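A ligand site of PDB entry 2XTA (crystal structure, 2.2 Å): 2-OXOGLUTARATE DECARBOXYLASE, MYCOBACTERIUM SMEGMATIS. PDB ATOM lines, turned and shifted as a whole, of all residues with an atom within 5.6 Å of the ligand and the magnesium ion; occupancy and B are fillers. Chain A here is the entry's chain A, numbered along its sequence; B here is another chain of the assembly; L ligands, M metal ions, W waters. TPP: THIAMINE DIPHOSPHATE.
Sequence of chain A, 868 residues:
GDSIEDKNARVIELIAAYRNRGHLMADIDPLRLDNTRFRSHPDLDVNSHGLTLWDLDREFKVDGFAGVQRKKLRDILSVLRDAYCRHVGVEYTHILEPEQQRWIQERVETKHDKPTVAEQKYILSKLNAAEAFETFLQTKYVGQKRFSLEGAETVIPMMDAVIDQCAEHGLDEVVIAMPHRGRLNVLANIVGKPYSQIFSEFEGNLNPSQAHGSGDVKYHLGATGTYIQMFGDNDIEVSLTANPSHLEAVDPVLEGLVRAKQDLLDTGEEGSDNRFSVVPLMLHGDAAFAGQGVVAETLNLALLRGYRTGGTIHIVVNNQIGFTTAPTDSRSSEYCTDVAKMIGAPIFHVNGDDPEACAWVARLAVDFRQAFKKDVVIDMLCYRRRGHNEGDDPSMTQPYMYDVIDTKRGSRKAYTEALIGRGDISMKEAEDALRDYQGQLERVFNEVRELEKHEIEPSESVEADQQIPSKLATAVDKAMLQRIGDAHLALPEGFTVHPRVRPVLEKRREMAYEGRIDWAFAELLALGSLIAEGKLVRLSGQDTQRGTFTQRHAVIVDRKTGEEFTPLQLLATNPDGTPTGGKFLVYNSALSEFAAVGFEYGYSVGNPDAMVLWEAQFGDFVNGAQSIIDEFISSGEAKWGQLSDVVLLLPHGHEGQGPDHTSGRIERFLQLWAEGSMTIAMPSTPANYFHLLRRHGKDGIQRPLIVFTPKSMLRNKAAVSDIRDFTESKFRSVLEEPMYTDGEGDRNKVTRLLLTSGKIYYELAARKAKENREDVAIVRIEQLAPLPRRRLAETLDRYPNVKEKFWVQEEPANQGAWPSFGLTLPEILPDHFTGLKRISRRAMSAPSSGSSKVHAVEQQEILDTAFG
Water W5 lies within hydrogen-bond range of the backbone carbonyl oxygen of Val 317 (2.6 Å), an oxygen (O3B) of the ligand (3.0 Å) and the backbone NH of Asp 286 (3.2 Å).
Water W1 lies within hydrogen-bond range of N of Phe 323 (2.8 Å), NH1 of Arg 384 (2.9 Å), O1B of the ligand (3.1 Å) and ND1 of His 388 (3.2 Å).
Water W3 bridges O of Phe 621 of chain B (2.6 Å) and OE2 of Glu 593 of chain B (3.1 Å).
The backbone NH (N) of Asp 286 sits close to an oxygen (O2A) of the ligand, at 3.4 Å.
N of Leu 247 is in hydrogen-bond range of N3' of the ligand (3.2 Å).
A ring nitrogen (NE2) of His 388 lies close to a sulfur (S1) of the ligand, 3.5 Å away.
The guanidinium group of Arg 181 lies within salt-bridge range of an oxygen (O3B) of the ligand, 2.9 Å away.
A nitrogen (N4') of the ligand sits at hydrogen-bond distance from the backbone carbonyl oxygen (O) of Ser 245 (2.8 Å).
The side-chain carboxylate (OE1) of Glu 593 of chain B lies within hydrogen-bond range of a nitrogen (N1') of the ligand (2.7 Å).
The backbone NH (N) of Ala 288 is in hydrogen-bond range of an oxygen (O1A) of the ligand (3.0 Å).
The backbone NH (N) of Ala 287 lies close to an oxygen (O2A) of the ligand, 3.0 Å away.
OE1 of Gln 617 of chain B lies close to N3 of the ligand (3.3 Å).
Merely in contact with the ligand: Gln 542 of chain B, Gly 322, Phe 621 of chain B, Leu 591 of chain B, Gly 285, His 246, Gln 292 and Phe 323.
Hydrophobic or aromatic side chains that line the ligand: Leu 247, Ala 287, Ala 288, His 388, Leu 591 of chain B and Phe 621 of chain B.
Of the 27 residues printed, 19 come within 4 Å of the ligand.
NH1 of Arg 384 lies within hydrogen-bond range of O of Phe 323 (2.9 Å).
NE2 of Gln 617 of chain B lies within hydrogen-bond range of OD2 of Asp 543 of chain B.
O of Leu 591 of chain B is in hydrogen-bond range of NE2 of Gln 292 (2.7 Å).
The backbone carbonyl oxygen (O) of Gln 542 of chain B lies within hydrogen-bond range of the side-chain amide nitrogen (NE2) of Gln 617 of chain B, at 3.2 Å.
The side-chain carboxylate (OD2) of Asp 286 lies close to the side-chain amide oxygen (OD1) of Asn 318 (3.4 Å).
The side-chain amide nitrogen (NE2) of Gln 292 lies within hydrogen-bond range of the side-chain carboxylate (OE2) of Glu 593 of chain B (3.1 Å).
The side-chain carboxylate (OE1) of Glu 593 of chain B is in hydrogen-bond range of the side-chain amide nitrogen (NE2) of Gln 542 of chain B, 2.8 Å away.
The magnesium ion is bound by an oxygen (O2A) of the ligand (2.0 Å), the backbone carbonyl oxygen of Ile 321 (2.0 Å), the side-chain amide oxygen of Asn 319 (2.1 Å), an oxygen (O2B) of the ligand (2.1 Å), water W5 (2.2 Å) and the side-chain carboxylate of Asp 286 (2.2 Å).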
ATOM      1  N   HIS A 180      18.410   6.876  21.829  1.00  0.00           N
ATOM      2  CA  HIS A 180      18.300   6.925  23.293  1.00  0.00           C
ATOM      3  C   HIS A 180      17.536   8.140  23.910  1.00  0.00           C
ATOM      4  O   HIS A 180      17.053   8.016  25.054  1.00  0.00           O
ATOM      5  CB  HIS A 180      19.683   6.840  23.942  1.00  0.00           C
ATOM      6  CG  HIS A 180      20.579   8.005  23.625  1.00  0.00           C
ATOM      7  ND1 HIS A 180      20.467   9.197  24.306  1.00  0.00           N
ATOM      8  CD2 HIS A 180      21.538   8.118  22.685  1.00  0.00           C
ATOM      9  CE1 HIS A 180      21.368  10.007  23.753  1.00  0.00           C
ATOM     10  NE2 HIS A 180      22.044   9.394  22.787  1.00  0.00           N
ATOM     11  N   ARG A 181      17.444   9.307  23.215  1.00  0.00           N
ATOM     12  CA  ARG A 181      16.785  10.499  23.778  1.00  0.00           C
ATOM     13  C   ARG A 181      15.289  10.245  24.105  1.00  0.00           C
ATOM     14  O   ARG A 181      14.495   9.965  23.222  1.00  0.00           O
ATOM     15  CB  ARG A 181      16.938  11.728  22.864  1.00  0.00           C
ATOM     16  CG  ARG A 181      16.437  13.026  23.512  1.00  0.00           C
ATOM     17  CD  ARG A 181      16.657  14.270  22.665  1.00  0.00           C
ATOM     18  NE  ARG A 181      18.062  14.447  22.217  1.00  0.00           N
ATOM     19  CZ  ARG A 181      19.042  14.887  23.003  1.00  0.00           C
ATOM     20  NH1 ARG A 181      18.801  15.179  24.272  1.00  0.00           N
ATOM     21  NH2 ARG A 181      20.262  15.034  22.519  1.00  0.00           N
ATOM     22  N   SER A 245      24.270   2.094  19.892  1.00  0.00           N
ATOM     23  CA  SER A 245      24.409   3.543  19.914  1.00  0.00           C
ATOM     24  C   SER A 245      24.493   4.085  18.462  1.00  0.00           C
ATOM     25  O   SER A 245      24.283   5.269  18.257  1.00  0.00           O
ATOM     26  CB  SER A 245      25.651   3.943  20.689  1.00  0.00           C
ATOM     27  OG  SER A 245      25.532   3.586  22.061  1.00  0.00           O
ATOM     28  N   HIS A 246      24.781   3.207  17.463  1.00  0.00           N
ATOM     29  CA  HIS A 246      24.862   3.557  16.029  1.00  0.00           C
ATOM     30  C   HIS A 246      23.509   4.007  15.570  1.00  0.00           C
ATOM     31  O   HIS A 246      22.578   3.201  15.487  1.00  0.00           O
ATOM     32  CB  HIS A 246      25.358   2.359  15.185  1.00  0.00           C
ATOM     33  CG  HIS A 246      26.780   1.977  15.461  1.00  0.00           C
ATOM     34  ND1 HIS A 246      27.223   1.679  16.742  1.00  0.00           N
ATOM     35  CD2 HIS A 246      27.813   1.867  14.588  1.00  0.00           C
ATOM     36  CE1 HIS A 246      28.517   1.410  16.620  1.00  0.00           C
ATOM     37  NE2 HIS A 246      28.917   1.480  15.351  1.00  0.00           N
ATOM     38  N   LEU A 247      23.368   5.323  15.393  1.00  0.00           N
ATOM     39  CA  LEU A 247      22.130   5.978  15.030  1.00  0.00           C
ATOM     40  C   LEU A 247      21.631   5.490  13.669  1.00  0.00           C
ATOM     41  O   LEU A 247      22.418   5.368  12.742  1.00  0.00           O
ATOM     42  CB  LEU A 247      22.304   7.520  15.024  1.00  0.00           C
ATOM     43  CG  LEU A 247      22.695   8.185  16.363  1.00  0.00           C
ATOM     44  CD1 LEU A 247      23.003   9.628  16.182  1.00  0.00           C
ATOM     45  CD2 LEU A 247      21.600   8.016  17.424  1.00  0.00           C
ATOM     46  N   GLY A 285      16.383  11.420  14.991  1.00  0.00           N
ATOM     47  CA  GLY A 285      16.959  12.728  15.281  1.00  0.00           C
ATOM     48  C   GLY A 285      17.201  13.395  13.924  1.00  0.00           C
ATOM     49  O   GLY A 285      17.351  12.686  12.912  1.00  0.00           O
ATOM     50  N   ASP A 286      17.267  14.746  13.897  1.00  0.00           N
ATOM     51  CA  ASP A 286      17.369  15.501  12.663  1.00  0.00           C
ATOM     52  C   ASP A 286      18.724  15.364  11.958  1.00  0.00           C
ATOM     53  O   ASP A 286      18.731  15.292  10.734  1.00  0.00           O
ATOM     54  CB  ASP A 286      17.046  17.012  12.891  1.00  0.00           C
ATOM     55  CG  ASP A 286      17.894  17.730  13.926  1.00  0.00           C
ATOM     56  OD1 ASP A 286      17.899  17.289  15.112  1.00  0.00           O
ATOM     57  OD2 ASP A 286      18.499  18.748  13.576  1.00  0.00           O
ATOM     58  N   ALA A 287      19.838  15.436  12.672  1.00  0.00           N
ATOM     59  CA  ALA A 287      21.159  15.328  12.035  1.00  0.00           C
ATOM     60  C   ALA A 287      21.374  13.885  11.485  1.00  0.00           C
ATOM     61  O   ALA A 287      21.815  13.746  10.349  1.00  0.00           O
ATOM     62  CB  ALA A 287      22.273  15.713  13.011  1.00  0.00           C
ATOM     63  N   ALA A 288      20.975  12.856  12.231  1.00  0.00           N
ATOM     64  CA  ALA A 288      21.115  11.444  11.835  1.00  0.00           C
ATOM     65  C   ALA A 288      20.201  11.045  10.657  1.00  0.00           C
ATOM     66  O   ALA A 288      20.613  10.267   9.810  1.00  0.00           O
ATOM     67  CB  ALA A 288      20.861  10.547  13.020  1.00  0.00           C
ATOM     68  N   PHE A 289      18.950  11.584  10.599  1.00  0.00           N
ATOM     69  CA  PHE A 289      17.985  11.277   9.534  1.00  0.00           C
ATOM     70  C   PHE A 289      18.494  11.776   8.190  1.00  0.00           C
ATOM     71  O   PHE A 289      18.248  11.147   7.161  1.00  0.00           O
ATOM     72  CB  PHE A 289      16.581  11.881   9.842  1.00  0.00           C
ATOM     73  CG  PHE A 289      15.453  11.280   9.032  1.00  0.00           C
ATOM     74  CD1 PHE A 289      15.013   9.979   9.252  1.00  0.00           C
ATOM     75  CD2 PHE A 289      14.826  12.016   8.032  1.00  0.00           C
ATOM     76  CE1 PHE A 289      13.971   9.429   8.508  1.00  0.00           C
ATOM     77  CE2 PHE A 289      13.782  11.469   7.275  1.00  0.00           C
ATOM     78  CZ  PHE A 289      13.365  10.171   7.515  1.00  0.00           C
ATOM     79  N   GLN A 292      22.643   9.680   7.540  1.00  0.00           N
ATOM     80  CA  GLN A 292      22.895   8.222   7.500  1.00  0.00           C
ATOM     81  C   GLN A 292      22.264   7.596   6.277  1.00  0.00           C
ATOM     82  O   GLN A 292      21.054   7.691   6.098  1.00  0.00           O
ATOM     83  CB  GLN A 292      22.394   7.541   8.782  1.00  0.00           C
ATOM     84  CG  GLN A 292      23.255   7.871  10.010  1.00  0.00           C
ATOM     85  CD  GLN A 292      24.619   7.204   9.962  1.00  0.00           C
ATOM     86  OE1 GLN A 292      24.725   5.976   9.857  1.00  0.00           O
ATOM     87  NE2 GLN A 292      25.674   7.990  10.070  1.00  0.00           N
ATOM     88  N   VAL A 317      12.487  13.891  15.756  1.00  0.00           N
ATOM     89  CA  VAL A 317      12.604  14.817  16.877  1.00  0.00           C
ATOM     90  C   VAL A 317      13.628  15.841  16.414  1.00  0.00           C
ATOM     91  O   VAL A 317      14.839  15.657  16.567  1.00  0.00           O
ATOM     92  CB  VAL A 317      12.975  14.096  18.202  1.00  0.00           C
ATOM     93  CG1 VAL A 317      13.083  15.088  19.353  1.00  0.00           C
ATOM     94  CG2 VAL A 317      11.957  12.994  18.524  1.00  0.00           C
ATOM     95  N   ASN A 318      13.138  16.879  15.731  1.00  0.00           N
ATOM     96  CA  ASN A 318      13.954  17.913  15.112  1.00  0.00           C
ATOM     97  C   ASN A 318      14.225  19.060  16.051  1.00  0.00           C
ATOM     98  O   ASN A 318      13.535  20.075  16.013  1.00  0.00           O
ATOM     99  CB  ASN A 318      13.282  18.400  13.825  1.00  0.00           C
ATOM    100  CG  ASN A 318      14.107  19.342  12.989  1.00  0.00           C
ATOM    101  OD1 ASN A 318      15.239  19.701  13.310  1.00  0.00           O
ATOM    102  ND2 ASN A 318      13.548  19.749  11.875  1.00  0.00           N
ATOM    103  N   ASN A 319      15.287  18.921  16.872  1.00  0.00           N
ATOM    104  CA  ASN A 319      15.688  19.935  17.862  1.00  0.00           C
ATOM    105  C   ASN A 319      16.709  20.908  17.264  1.00  0.00           C
ATOM    106  O   ASN A 319      17.329  21.698  17.984  1.00  0.00           O
ATOM    107  CB  ASN A 319      16.212  19.297  19.142  1.00  0.00           C
ATOM    108  CG  ASN A 319      17.302  18.271  18.971  1.00  0.00           C
ATOM    109  OD1 ASN A 319      17.951  18.191  17.909  1.00  0.00           O
ATOM    110  ND2 ASN A 319      17.524  17.483  20.029  1.00  0.00           N
ATOM    111  N   GLN A 320      16.863  20.842  15.915  1.00  0.00           N
ATOM    112  CA  GLN A 320      17.626  21.752  15.058  1.00  0.00           C
ATOM    113  C   GLN A 320      19.090  21.900  15.499  1.00  0.00           C
ATOM    114  O   GLN A 320      19.661  23.001  15.505  1.00  0.00           O
ATOM    115  CB  GLN A 320      16.927  23.139  15.041  1.00  0.00           C
ATOM    116  CG  GLN A 320      15.399  23.066  14.762  1.00  0.00           C
ATOM    117  CD  GLN A 320      14.725  24.396  15.043  1.00  0.00           C
ATOM    118  OE1 GLN A 320      15.212  25.454  14.643  1.00  0.00           O
ATOM    119  NE2 GLN A 320      13.608  24.393  15.771  1.00  0.00           N
ATOM    120  N   ILE A 321      19.691  20.752  15.883  1.00  0.00           N
ATOM    121  CA  ILE A 321      21.051  20.629  16.403  1.00  0.00           C
ATOM    122  C   ILE A 321      21.406  19.157  16.470  1.00  0.00           C
ATOM    123  O   ILE A 321      20.546  18.288  16.649  1.00  0.00           O
ATOM    124  CB  ILE A 321      21.245  21.359  17.801  1.00  0.00           C
ATOM    125  CG1 ILE A 321      22.730  21.651  18.110  1.00  0.00           C
ATOM    126  CG2 ILE A 321      20.452  20.715  19.002  1.00  0.00           C
ATOM    127  CD1 ILE A 321      22.937  22.677  19.169  1.00  0.00           C
ATOM    128  N   GLY A 322      22.679  18.905  16.267  1.00  0.00           N
ATOM    129  CA  GLY A 322      23.270  17.567  16.321  1.00  0.00           C
ATOM    130  C   GLY A 322      24.542  17.710  17.118  1.00  0.00           C
ATOM    131  O   GLY A 322      25.564  18.110  16.559  1.00  0.00           O
ATOM    132  N   PHE A 323      24.445  17.511  18.456  1.00  0.00           N
ATOM    133  CA  PHE A 323      25.552  17.686  19.403  1.00  0.00           C
ATOM    134  C   PHE A 323      25.981  19.174  19.421  1.00  0.00           C
ATOM    135  O   PHE A 323      25.304  19.959  20.060  1.00  0.00           O
ATOM    136  CB  PHE A 323      26.737  16.714  19.115  1.00  0.00           C
ATOM    137  CG  PHE A 323      27.699  16.426  20.258  1.00  0.00           C
ATOM    138  CD1 PHE A 323      27.921  17.374  21.248  1.00  0.00           C
ATOM    139  CD2 PHE A 323      28.416  15.234  20.314  1.00  0.00           C
ATOM    140  CE1 PHE A 323      28.811  17.119  22.304  1.00  0.00           C
ATOM    141  CE2 PHE A 323      29.313  14.990  21.350  1.00  0.00           C
ATOM    142  CZ  PHE A 323      29.516  15.924  22.339  1.00  0.00           C
ATOM    143  N   ARG A 384      16.524  21.401  22.244  1.00  0.00           N
ATOM    144  CA  ARG A 384      17.193  20.585  23.243  1.00  0.00           C
ATOM    145  C   ARG A 384      17.593  21.525  24.378  1.00  0.00           C
ATOM    146  O   ARG A 384      18.483  22.344  24.192  1.00  0.00           O
ATOM    147  CB  ARG A 384      18.398  19.877  22.566  1.00  0.00           C
ATOM    148  CG  ARG A 384      19.108  18.821  23.408  1.00  0.00           C
ATOM    149  CD  ARG A 384      20.489  18.586  22.824  1.00  0.00           C
ATOM    150  NE  ARG A 384      21.391  19.681  23.176  1.00  0.00           N
ATOM    151  CZ  ARG A 384      22.472  20.030  22.489  1.00  0.00           C
ATOM    152  NH1 ARG A 384      22.812  19.383  21.395  1.00  0.00           N
ATOM    153  NH2 ARG A 384      23.209  21.064  22.884  1.00  0.00           N
ATOM    154  N   HIS A 388      24.418  18.612  25.205  1.00  0.00           N
ATOM    155  CA  HIS A 388      24.330  17.262  24.681  1.00  0.00           C
ATOM    156  C   HIS A 388      24.633  16.210  25.761  1.00  0.00           C
ATOM    157  O   HIS A 388      23.972  15.161  25.777  1.00  0.00           O
ATOM    158  CB  HIS A 388      25.302  17.126  23.519  1.00  0.00           C
ATOM    159  CG  HIS A 388      25.113  15.865  22.743  1.00  0.00           C
ATOM    160  ND1 HIS A 388      24.045  15.724  21.878  1.00  0.00           N
ATOM    161  CD2 HIS A 388      25.852  14.744  22.738  1.00  0.00           C
ATOM    162  CE1 HIS A 388      24.185  14.520  21.359  1.00  0.00           C
ATOM    163  NE2 HIS A 388      25.245  13.894  21.851  1.00  0.00           N
ATOM    164  N   GLN B 542      32.892  14.523  13.131  1.00  0.00           N
ATOM    165  CA  GLN B 542      31.694  14.950  13.872  1.00  0.00           C
ATOM    166  C   GLN B 542      32.077  15.769  15.099  1.00  0.00           C
ATOM    167  O   GLN B 542      32.830  15.277  15.939  1.00  0.00           O
ATOM    168  CB  GLN B 542      30.838  13.746  14.270  1.00  0.00           C
ATOM    169  CG  GLN B 542      30.020  13.195  13.100  1.00  0.00           C
ATOM    170  CD  GLN B 542      29.779  11.718  13.237  1.00  0.00           C
ATOM    171  OE1 GLN B 542      29.856  11.148  14.322  1.00  0.00           O
ATOM    172  NE2 GLN B 542      29.503  11.065  12.120  1.00  0.00           N
ATOM    173  N   ASP B 543      31.649  17.046  15.129  1.00  0.00           N
ATOM    174  CA  ASP B 543      31.933  17.994  16.221  1.00  0.00           C
ATOM    175  C   ASP B 543      33.442  18.229  16.457  1.00  0.00           C
ATOM    176  O   ASP B 543      33.857  18.559  17.570  1.00  0.00           O
ATOM    177  CB  ASP B 543      31.236  17.532  17.522  1.00  0.00           C
ATOM    178  CG  ASP B 543      29.759  17.267  17.291  1.00  0.00           C
ATOM    179  OD1 ASP B 543      29.004  18.255  17.109  1.00  0.00           O
ATOM    180  OD2 ASP B 543      29.388  16.085  17.164  1.00  0.00           O
ATOM    181  N   LEU B 591      26.457  13.894   9.768  1.00  0.00           N
ATOM    182  CA  LEU B 591      26.454  12.687  10.582  1.00  0.00           C
ATOM    183  C   LEU B 591      26.580  11.460   9.659  1.00  0.00           C
ATOM    184  O   LEU B 591      25.632  10.680   9.525  1.00  0.00           O
ATOM    185  CB  LEU B 591      25.196  12.633  11.475  1.00  0.00           C
ATOM    186  CG  LEU B 591      25.367  11.976  12.836  1.00  0.00           C
ATOM    187  CD1 LEU B 591      24.250  12.344  13.752  1.00  0.00           C
ATOM    188  CD2 LEU B 591      25.494  10.416  12.731  1.00  0.00           C
ATOM    189  N   GLU B 593      29.652   8.433   8.219  1.00  0.00           N
ATOM    190  CA  GLU B 593      30.957   7.817   8.371  1.00  0.00           C
ATOM    191  C   GLU B 593      31.430   7.405   6.991  1.00  0.00           C
ATOM    192  O   GLU B 593      32.488   7.833   6.579  1.00  0.00           O
ATOM    193  CB  GLU B 593      30.942   6.629   9.365  1.00  0.00           C
ATOM    194  CG  GLU B 593      30.858   7.093  10.819  1.00  0.00           C
ATOM    195  CD  GLU B 593      29.474   7.453  11.321  1.00  0.00           C
ATOM    196  OE1 GLU B 593      29.368   8.301  12.226  1.00  0.00           O
ATOM    197  OE2 GLU B 593      28.488   6.891  10.808  1.00  0.00           O
ATOM    198  N   GLN B 617      33.811  10.196  16.034  1.00  0.00           N
ATOM    199  CA  GLN B 617      33.313  10.708  17.314  1.00  0.00           C
ATOM    200  C   GLN B 617      33.876   9.790  18.414  1.00  0.00           C
ATOM    201  O   GLN B 617      34.465  10.244  19.394  1.00  0.00           O
ATOM    202  CB  GLN B 617      31.770  10.785  17.309  1.00  0.00           C
ATOM    203  CG  GLN B 617      31.200  11.370  18.584  1.00  0.00           C
ATOM    204  CD  GLN B 617      30.371  12.601  18.346  1.00  0.00           C
ATOM    205  OE1 GLN B 617      29.147  12.580  18.471  1.00  0.00           O
ATOM    206  NE2 GLN B 617      31.030  13.714  18.061  1.00  0.00           N
ATOM    207  N   PHE B 621      32.345   3.821  15.771  1.00  0.00           N
ATOM    208  CA  PHE B 621      31.466   4.188  14.665  1.00  0.00           C
ATOM    209  C   PHE B 621      32.143   4.127  13.313  1.00  0.00           C
ATOM    210  O   PHE B 621      31.434   4.200  12.299  1.00  0.00           O
ATOM    211  CB  PHE B 621      30.875   5.594  14.901  1.00  0.00           C
ATOM    212  CG  PHE B 621      30.078   5.693  16.180  1.00  0.00           C
ATOM    213  CD1 PHE B 621      30.466   6.573  17.187  1.00  0.00           C
ATOM    214  CD2 PHE B 621      28.958   4.897  16.384  1.00  0.00           C
ATOM    215  CE1 PHE B 621      29.752   6.644  18.392  1.00  0.00           C
ATOM    216  CE2 PHE B 621      28.244   4.968  17.589  1.00  0.00           C
ATOM    217  CZ  PHE B 621      28.650   5.843  18.585  1.00  0.00           C
ATOM    218  N   HIS B 661      31.292   2.637  22.898  1.00  0.00           N
ATOM    219  CA  HIS B 661      32.088   3.797  23.313  1.00  0.00           C
ATOM    220  C   HIS B 661      33.362   3.287  23.949  1.00  0.00           C
ATOM    221  O   HIS B 661      33.830   3.828  24.955  1.00  0.00           O
ATOM    222  CB  HIS B 661      31.282   4.699  24.283  1.00  0.00           C
ATOM    223  CG  HIS B 661      30.083   5.295  23.619  1.00  0.00           C
ATOM    224  ND1 HIS B 661      28.868   4.657  23.656  1.00  0.00           N
ATOM    225  CD2 HIS B 661      29.993   6.399  22.845  1.00  0.00           C
ATOM    226  CE1 HIS B 661      28.059   5.401  22.919  1.00  0.00           C
ATOM    227  NE2 HIS B 661      28.686   6.472  22.425  1.00  0.00           N
HETATM  228  N1' TPP L   1      27.586   8.083  14.245  1.00  0.00           N
HETATM  229  C2' TPP L   1      26.707   7.118  14.406  1.00  0.00           C
HETATM  230  CM2 TPP L   1      26.385   6.197  13.252  1.00  0.00           C
HETATM  231  N3' TPP L   1      26.106   6.954  15.562  1.00  0.00           N
HETATM  232  C4' TPP L   1      26.410   7.745  16.611  1.00  0.00           C
HETATM  233  N4' TPP L   1      25.809   7.522  17.842  1.00  0.00           N
HETATM  234  C5' TPP L   1      27.319   8.791  16.479  1.00  0.00           C
HETATM  235  C6' TPP L   1      27.880   8.947  15.223  1.00  0.00           C
HETATM  236  C7' TPP L   1      27.649   9.751  17.618  1.00  0.00           C
HETATM  237  N3  TPP L   1      26.533  10.671  17.981  1.00  0.00           N
HETATM  238  C2  TPP L   1      25.844  10.473  19.061  1.00  0.00           C
HETATM  239  S1  TPP L   1      24.643  11.678  19.269  1.00  0.00           S
HETATM  240  C5  TPP L   1      25.201  12.497  17.820  1.00  0.00           C
HETATM  241  C4  TPP L   1      26.213  11.767  17.306  1.00  0.00           C
HETATM  242  CM4 TPP L   1      26.873  12.231  16.031  1.00  0.00           C
HETATM  243  C6  TPP L   1      24.511  13.747  17.293  1.00  0.00           C
HETATM  244  C7  TPP L   1      23.055  13.350  17.038  1.00  0.00           C
HETATM  245  O7  TPP L   1      22.309  14.340  16.303  1.00  0.00           O
HETATM  246  PA  TPP L   1      20.724  14.172  16.126  1.00  0.00           P
HETATM  247  O1A TPP L   1      20.451  13.069  15.183  1.00  0.00           O
HETATM  248  O2A TPP L   1      20.053  15.552  15.632  1.00  0.00           O
HETATM  249  O3A TPP L   1      20.144  13.763  17.585  1.00  0.00           O
HETATM  250  PB  TPP L   1      19.924  14.497  18.887  1.00  0.00           P
HETATM  251  O1B TPP L   1      21.068  14.130  19.933  1.00  0.00           O
HETATM  252  O2B TPP L   1      19.890  15.970  18.622  1.00  0.00           O
HETATM  253  O3B TPP L   1      18.454  14.122  19.410  1.00  0.00           O
HETATM  254 MG    MG M   1      19.154  16.838  16.862  1.00  0.00          MG
HETATM  255  O   HOH W   1      22.063  17.115  19.831  1.00  0.00           O
HETATM  256  O   HOH W   2      19.640  10.753  16.664  1.00  0.00           O
HETATM  257  O   HOH W   3      28.855   4.077  11.980  1.00  0.00           O
HETATM  258  O   HOH W   4      17.668  11.625  18.718  1.00  0.00           O
HETATM  259  O   HOH W   5      17.388  15.572  17.013  1.00  0.00           O
